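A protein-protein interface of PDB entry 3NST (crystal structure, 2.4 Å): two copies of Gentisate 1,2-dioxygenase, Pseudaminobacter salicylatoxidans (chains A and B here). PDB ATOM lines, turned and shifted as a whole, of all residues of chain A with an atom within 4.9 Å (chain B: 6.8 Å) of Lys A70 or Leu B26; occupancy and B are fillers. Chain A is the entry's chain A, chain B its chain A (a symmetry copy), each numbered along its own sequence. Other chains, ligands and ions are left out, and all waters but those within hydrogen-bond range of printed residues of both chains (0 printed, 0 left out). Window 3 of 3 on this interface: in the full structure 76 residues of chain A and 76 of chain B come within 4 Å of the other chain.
The backbone carbonyl oxygen (O) of Leu A67 lies within hydrogen-bond range of the side-chain hydroxyl (OG) of Ser A71 (2.8 Å).
OE1 of Glu A73 is in salt-bridge range of NZ of Lys A70 (3.1 Å).
NE1 of Trp B39 is in hydrogen-bond range of OH of Tyr B27 (3.1 Å).
Leu A67 touches Leu B26 (O to CD1, 3.9 Å).
Ser B29 touches Leu A67.
Leu A67 touches Phe B30 (CD1 to CD1, 3.9 Å).
Leu B26 touches Lys A70.
Ser A71 touches Leu B26.
Ser A71 touches Phe B30.
Trp B39 touches Ser A71 (CH2 to OG, 3.6 Å).
CD1 of Leu A74 touches O of Glu B22, 3.5 Å away.
Leu B26 touches Leu A74.
CG2 of Val A75 touches CZ2 of Trp B39 (3.6 Å).
Printed residues of chain A within 4 Å of Leu B26: Leu A67, Lys A70, Ser A71 and Leu A74.
Printed residues of chain A within 4 Å of Pro B17: Leu A74 (3.6 Å).
Printed residues of chain A within 4 Å of Phe B30: Leu A67 and Ser A71.
Of the printed residues of chain A, Ser B29 touches Leu A67 (3.7 Å).
The nearest printed residue of chain A that does not touch Leu B26 is Val A75 (4.4 Å).
Hydrophobic or aromatic side chains of chain A that line the printed part of chain B: Leu A67, Leu A74 and Val A75.
Of the 13 printed residues of chain B, 7 touch a printed residue of chain A.
Hydrophobic or aromatic side chains of chain B within 4 Å of the printed part of chain A: Pro B17, Leu B26, Phe B30 and Trp B39.
Among the printed residues, 12 pairs touch across the chains.
Among the printed residues, no Asp or Glu carboxylate lies within 4 Å of a Lys or Arg side-chain nitrogen of the other chain.
No position is printed for both chains.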
ATOM      1  N   ARG A  66      -0.642  13.369   4.451  1.00  0.00           N
ATOM      2  CA  ARG A  66       0.157  14.280   5.295  1.00  0.00           C
ATOM      3  C   ARG A  66       0.507  13.628   6.658  1.00  0.00           C
ATOM      4  O   ARG A  66       1.659  13.755   7.145  1.00  0.00           O
ATOM      5  CB  ARG A  66      -0.534  15.635   5.504  1.00  0.00           C
ATOM      6  CG  ARG A  66       0.121  16.509   6.575  1.00  0.00           C
ATOM      7  CD  ARG A  66      -0.616  17.864   6.837  1.00  0.00           C
ATOM      8  NE  ARG A  66      -2.064  17.755   7.040  1.00  0.00           N
ATOM      9  CZ  ARG A  66      -2.698  17.530   8.208  1.00  0.00           C
ATOM     10  NH1 ARG A  66      -2.020  17.364   9.362  1.00  0.00           N
ATOM     11  NH2 ARG A  66      -4.042  17.451   8.221  1.00  0.00           N
ATOM     12  N   LEU A  67      -0.483  12.956   7.254  1.00  0.00           N
ATOM     13  CA  LEU A  67      -0.292  12.240   8.527  1.00  0.00           C
ATOM     14  C   LEU A  67       0.615  11.014   8.355  1.00  0.00           C
ATOM     15  O   LEU A  67       1.361  10.645   9.283  1.00  0.00           O
ATOM     16  CB  LEU A  67      -1.634  11.813   9.110  1.00  0.00           C
ATOM     17  CG  LEU A  67      -2.511  12.944   9.622  1.00  0.00           C
ATOM     18  CD1 LEU A  67      -3.740  12.382  10.256  1.00  0.00           C
ATOM     19  CD2 LEU A  67      -1.746  13.805  10.611  1.00  0.00           C
ATOM     20  N   ALA A  68       0.539  10.374   7.189  1.00  0.00           N
ATOM     21  CA  ALA A  68       1.447   9.292   6.877  1.00  0.00           C
ATOM     22  C   ALA A  68       2.910   9.768   6.739  1.00  0.00           C
ATOM     23  O   ALA A  68       3.802   9.124   7.271  1.00  0.00           O
ATOM     24  CB  ALA A  68       0.990   8.539   5.636  1.00  0.00           C
ATOM     25  N   ARG A  69       3.155  10.856   6.012  1.00  0.00           N
ATOM     26  CA  ARG A  69       4.499  11.408   5.871  1.00  0.00           C
ATOM     27  C   ARG A  69       5.085  11.748   7.253  1.00  0.00           C
ATOM     28  O   ARG A  69       6.260  11.445   7.548  1.00  0.00           O
ATOM     29  CB  ARG A  69       4.486  12.635   4.943  1.00  0.00           C
ATOM     30  CG  ARG A  69       4.508  12.282   3.441  1.00  0.00           C
ATOM     31  CD  ARG A  69       3.917  13.374   2.485  1.00  0.00           C
ATOM     32  NE  ARG A  69       4.087  13.005   1.075  1.00  0.00           N
ATOM     33  CZ  ARG A  69       3.866  13.813   0.036  1.00  0.00           C
ATOM     34  NH1 ARG A  69       3.412  15.065   0.228  1.00  0.00           N
ATOM     35  NH2 ARG A  69       4.072  13.356  -1.209  1.00  0.00           N
ATOM     36  N   LYS A  70       4.263  12.358   8.111  1.00  0.00           N
ATOM     37  CA  LYS A  70       4.747  12.751   9.408  1.00  0.00           C
ATOM     38  C   LYS A  70       5.101  11.497  10.221  1.00  0.00           C
ATOM     39  O   LYS A  70       6.185  11.425  10.820  1.00  0.00           O
ATOM     40  CB  LYS A  70       3.754  13.695  10.068  1.00  0.00           C
ATOM     41  CG  LYS A  70       4.091  14.210  11.492  1.00  0.00           C
ATOM     42  CD  LYS A  70       5.334  15.066  11.574  1.00  0.00           C
ATOM     43  CE  LYS A  70       5.161  16.410  10.902  1.00  0.00           C
ATOM     44  NZ  LYS A  70       6.505  16.890  10.396  1.00  0.00           N
ATOM     45  N   SER A  71       4.258  10.473  10.166  1.00  0.00           N
ATOM     46  CA  SER A  71       4.581   9.204  10.787  1.00  0.00           C
ATOM     47  C   SER A  71       5.912   8.621  10.269  1.00  0.00           C
ATOM     48  O   SER A  71       6.593   7.946  11.006  1.00  0.00           O
ATOM     49  CB  SER A  71       3.456   8.187  10.573  1.00  0.00           C
ATOM     50  OG  SER A  71       2.240   8.716  11.075  1.00  0.00           O
ATOM     51  N   GLY A  72       6.234   8.854   8.995  1.00  0.00           N
ATOM     52  CA  GLY A  72       7.516   8.471   8.430  1.00  0.00           C
ATOM     53  C   GLY A  72       8.698   9.144   9.148  1.00  0.00           C
ATOM     54  O   GLY A  72       9.705   8.514   9.369  1.00  0.00           O
ATOM     55  N   GLU A  73       8.542  10.415   9.523  1.00  0.00           N
ATOM     56  CA  GLU A  73       9.600  11.161  10.194  1.00  0.00           C
ATOM     57  C   GLU A  73       9.683  10.757  11.640  1.00  0.00           C
ATOM     58  O   GLU A  73      10.784  10.526  12.160  1.00  0.00           O
ATOM     59  CB  GLU A  73       9.329  12.655  10.189  1.00  0.00           C
ATOM     60  CG  GLU A  73       9.251  13.260   8.813  1.00  0.00           C
ATOM     61  CD  GLU A  73       8.834  14.695   8.937  1.00  0.00           C
ATOM     62  OE1 GLU A  73       9.178  15.283   9.999  1.00  0.00           O
ATOM     63  OE2 GLU A  73       8.164  15.222   8.014  1.00  0.00           O
ATOM     64  N   LEU A  74       8.527  10.685  12.303  1.00  0.00           N
ATOM     65  CA  LEU A  74       8.528  10.568  13.735  1.00  0.00           C
ATOM     66  C   LEU A  74       8.674   9.139  14.188  1.00  0.00           C
ATOM     67  O   LEU A  74       8.960   8.914  15.361  1.00  0.00           O
ATOM     68  CB  LEU A  74       7.290  11.213  14.345  1.00  0.00           C
ATOM     69  CG  LEU A  74       7.151  12.685  14.028  1.00  0.00           C
ATOM     70  CD1 LEU A  74       6.088  13.323  14.842  1.00  0.00           C
ATOM     71  CD2 LEU A  74       8.492  13.407  14.273  1.00  0.00           C
ATOM     72  N   VAL A  75       8.478   8.160  13.308  1.00  0.00           N
ATOM     73  CA  VAL A  75       8.277   6.788  13.798  1.00  0.00           C
ATOM     74  C   VAL A  75       9.175   5.890  13.004  1.00  0.00           C
ATOM     75  O   VAL A  75       8.746   5.341  12.004  1.00  0.00           O
ATOM     76  CB  VAL A  75       6.803   6.347  13.651  1.00  0.00           C
ATOM     77  CG1 VAL A  75       6.608   4.952  14.151  1.00  0.00           C
ATOM     78  CG2 VAL A  75       5.817   7.367  14.370  1.00  0.00           C
ATOM     79  N   PRO B  17       7.719   5.369  19.630  1.00  0.00           N
ATOM     80  CA  PRO B  17       8.436   6.579  19.153  1.00  0.00           C
ATOM     81  C   PRO B  17       8.762   7.563  20.284  1.00  0.00           C
ATOM     82  O   PRO B  17       8.145   7.499  21.351  1.00  0.00           O
ATOM     83  CB  PRO B  17       7.451   7.222  18.135  1.00  0.00           C
ATOM     84  CG  PRO B  17       6.174   6.597  18.376  1.00  0.00           C
ATOM     85  CD  PRO B  17       6.407   5.226  18.973  1.00  0.00           C
ATOM     86  N   PRO B  21       7.000  16.980  21.632  1.00  0.00           N
ATOM     87  CA  PRO B  21       5.766  17.716  21.350  1.00  0.00           C
ATOM     88  C   PRO B  21       5.184  17.415  19.937  1.00  0.00           C
ATOM     89  O   PRO B  21       3.963  17.443  19.762  1.00  0.00           O
ATOM     90  CB  PRO B  21       6.182  19.203  21.512  1.00  0.00           C
ATOM     91  CG  PRO B  21       7.378  19.141  22.466  1.00  0.00           C
ATOM     92  CD  PRO B  21       8.081  17.867  22.125  1.00  0.00           C
ATOM     93  N   GLU B  22       6.050  17.117  18.979  1.00  0.00           N
ATOM     94  CA  GLU B  22       5.634  16.773  17.632  1.00  0.00           C
ATOM     95  C   GLU B  22       4.867  15.394  17.607  1.00  0.00           C
ATOM     96  O   GLU B  22       3.907  15.217  16.810  1.00  0.00           O
ATOM     97  CB  GLU B  22       6.839  16.718  16.690  1.00  0.00           C
ATOM     98  CG  GLU B  22       7.579  18.048  16.455  1.00  0.00           C
ATOM     99  CD  GLU B  22       8.550  18.497  17.631  1.00  0.00           C
ATOM    100  OE1 GLU B  22       9.055  19.634  17.505  1.00  0.00           O
ATOM    101  OE2 GLU B  22       8.806  17.775  18.653  1.00  0.00           O
ATOM    102  N   LEU B  23       5.276  14.448  18.475  1.00  0.00           N
ATOM    103  CA  LEU B  23       4.622  13.165  18.484  1.00  0.00           C
ATOM    104  C   LEU B  23       3.216  13.341  19.071  1.00  0.00           C
ATOM    105  O   LEU B  23       2.286  12.605  18.672  1.00  0.00           O
ATOM    106  CB  LEU B  23       5.423  12.095  19.221  1.00  0.00           C
ATOM    107  CG  LEU B  23       4.724  10.728  19.104  1.00  0.00           C
ATOM    108  CD1 LEU B  23       4.878  10.106  17.689  1.00  0.00           C
ATOM    109  CD2 LEU B  23       5.089   9.678  20.221  1.00  0.00           C
ATOM    110  N   ARG B  24       3.074  14.315  19.985  1.00  0.00           N
ATOM    111  CA  ARG B  24       1.860  14.506  20.699  1.00  0.00           C
ATOM    112  C   ARG B  24       0.873  15.268  19.791  1.00  0.00           C
ATOM    113  O   ARG B  24      -0.327  14.994  19.831  1.00  0.00           O
ATOM    114  CB  ARG B  24       2.079  15.228  22.078  1.00  0.00           C
ATOM    115  CG  ARG B  24       2.729  14.336  23.174  1.00  0.00           C
ATOM    116  CD  ARG B  24       2.714  14.934  24.615  1.00  0.00           C
ATOM    117  NE  ARG B  24       3.553  16.137  24.761  1.00  0.00           N
ATOM    118  CZ  ARG B  24       4.884  16.135  24.966  1.00  0.00           C
ATOM    119  NH1 ARG B  24       5.586  14.990  25.022  1.00  0.00           N
ATOM    120  NH2 ARG B  24       5.529  17.291  25.094  1.00  0.00           N
ATOM    121  N   ALA B  25       1.396  16.224  19.011  1.00  0.00           N
ATOM    122  CA  ALA B  25       0.662  16.892  17.959  1.00  0.00           C
ATOM    123  C   ALA B  25       0.202  15.864  16.909  1.00  0.00           C
ATOM    124  O   ALA B  25      -0.992  15.842  16.616  1.00  0.00           O
ATOM    125  CB  ALA B  25       1.444  18.086  17.320  1.00  0.00           C
ATOM    126  N   LEU B  26       1.093  15.004  16.394  1.00  0.00           N
ATOM    127  CA  LEU B  26       0.678  13.871  15.520  1.00  0.00           C
ATOM    128  C   LEU B  26      -0.523  13.084  16.096  1.00  0.00           C
ATOM    129  O   LEU B  26      -1.484  12.785  15.388  1.00  0.00           O
ATOM    130  CB  LEU B  26       1.857  12.926  15.182  1.00  0.00           C
ATOM    131  CG  LEU B  26       1.752  11.689  14.243  1.00  0.00           C
ATOM    132  CD1 LEU B  26       1.414  12.150  12.864  1.00  0.00           C
ATOM    133  CD2 LEU B  26       3.069  10.823  14.121  1.00  0.00           C
ATOM    134  N   TYR B  27      -0.486  12.796  17.388  1.00  0.00           N
ATOM    135  CA  TYR B  27      -1.483  11.940  17.975  1.00  0.00           C
ATOM    136  C   TYR B  27      -2.774  12.696  18.168  1.00  0.00           C
ATOM    137  O   TYR B  27      -3.843  12.098  18.116  1.00  0.00           O
ATOM    138  CB  TYR B  27      -1.026  11.339  19.319  1.00  0.00           C
ATOM    139  CG  TYR B  27       0.001  10.239  19.222  1.00  0.00           C
ATOM    140  CD1 TYR B  27       0.382   9.679  18.006  1.00  0.00           C
ATOM    141  CD2 TYR B  27       0.562   9.704  20.375  1.00  0.00           C
ATOM    142  CE1 TYR B  27       1.317   8.628  17.944  1.00  0.00           C
ATOM    143  CE2 TYR B  27       1.504   8.656  20.316  1.00  0.00           C
ATOM    144  CZ  TYR B  27       1.873   8.140  19.108  1.00  0.00           C
ATOM    145  OH  TYR B  27       2.810   7.114  19.117  1.00  0.00           O
ATOM    146  N   LYS B  28      -2.677  13.991  18.437  1.00  0.00           N
ATOM    147  CA  LYS B  28      -3.889  14.767  18.533  1.00  0.00           C
ATOM    148  C   LYS B  28      -4.555  14.942  17.147  1.00  0.00           C
ATOM    149  O   LYS B  28      -5.794  14.926  17.070  1.00  0.00           O
ATOM    150  CB  LYS B  28      -3.706  16.096  19.320  1.00  0.00           C
ATOM    151  CG  LYS B  28      -4.772  17.192  18.985  1.00  0.00           C
ATOM    152  CD  LYS B  28      -5.142  18.091  20.188  1.00  0.00           C
ATOM    153  CE  LYS B  28      -5.395  19.607  19.745  1.00  0.00           C
ATOM    154  NZ  LYS B  28      -5.385  20.551  20.920  1.00  0.00           N
ATOM    155  N   SER B  29      -3.751  15.035  16.081  1.00  0.00           N
ATOM    156  CA  SER B  29      -4.306  15.028  14.728  1.00  0.00           C
ATOM    157  C   SER B  29      -4.989  13.728  14.462  1.00  0.00           C
ATOM    158  O   SER B  29      -6.121  13.766  13.933  1.00  0.00           O
ATOM    159  CB  SER B  29      -3.306  15.233  13.630  1.00  0.00           C
ATOM    160  OG  SER B  29      -2.845  16.546  13.690  1.00  0.00           O
ATOM    161  N   PHE B  30      -4.355  12.602  14.863  1.00  0.00           N
ATOM    162  CA  PHE B  30      -5.012  11.243  14.750  1.00  0.00           C
ATOM    163  C   PHE B  30      -6.421  11.208  15.318  1.00  0.00           C
ATOM    164  O   PHE B  30      -7.349  10.751  14.623  1.00  0.00           O
ATOM    165  CB  PHE B  30      -4.205  10.049  15.346  1.00  0.00           C
ATOM    166  CG  PHE B  30      -2.945   9.703  14.574  1.00  0.00           C
ATOM    167  CD1 PHE B  30      -2.801  10.057  13.252  1.00  0.00           C
ATOM    168  CD2 PHE B  30      -1.936   8.977  15.175  1.00  0.00           C
ATOM    169  CE1 PHE B  30      -1.649   9.712  12.557  1.00  0.00           C
ATOM    170  CE2 PHE B  30      -0.808   8.629  14.503  1.00  0.00           C
ATOM    171  CZ  PHE B  30      -0.632   8.993  13.214  1.00  0.00           C
ATOM    172  N   GLU B  31      -6.552  11.617  16.581  1.00  0.00           N
ATOM    173  CA  GLU B  31      -7.840  11.595  17.290  1.00  0.00           C
ATOM    174  C   GLU B  31      -8.812  12.437  16.484  1.00  0.00           C
ATOM    175  O   GLU B  31      -9.944  12.054  16.292  1.00  0.00           O
ATOM    176  CB  GLU B  31      -7.715  12.150  18.729  1.00  0.00           C
ATOM    177  CG  GLU B  31      -9.064  12.590  19.386  1.00  0.00           C
ATOM    178  CD  GLU B  31      -8.904  13.565  20.581  1.00  0.00           C
ATOM    179  OE1 GLU B  31      -9.241  13.136  21.712  1.00  0.00           O
ATOM    180  OE2 GLU B  31      -8.457  14.743  20.397  1.00  0.00           O
ATOM    181  N   TRP B  39       0.864   0.870  15.539  1.00  0.00           N
ATOM    182  CA  TRP B  39       2.046   0.602  16.401  1.00  0.00           C
ATOM    183  C   TRP B  39       1.806   0.834  17.889  1.00  0.00           C
ATOM    184  O   TRP B  39       2.729   0.727  18.707  1.00  0.00           O
ATOM    185  CB  TRP B  39       3.273   1.405  15.961  1.00  0.00           C
ATOM    186  CG  TRP B  39       3.116   2.892  16.081  1.00  0.00           C
ATOM    187  CD1 TRP B  39       3.315   3.639  17.187  1.00  0.00           C
ATOM    188  CD2 TRP B  39       2.711   3.818  15.039  1.00  0.00           C
ATOM    189  NE1 TRP B  39       3.050   4.987  16.918  1.00  0.00           N
ATOM    190  CE2 TRP B  39       2.700   5.114  15.602  1.00  0.00           C
ATOM    191  CE3 TRP B  39       2.367   3.672  13.698  1.00  0.00           C
ATOM    192  CZ2 TRP B  39       2.376   6.254  14.863  1.00  0.00           C
ATOM    193  CZ3 TRP B  39       2.046   4.810  12.963  1.00  0.00           C
ATOM    194  CH2 TRP B  39       2.060   6.069  13.549  1.00  0.00           C
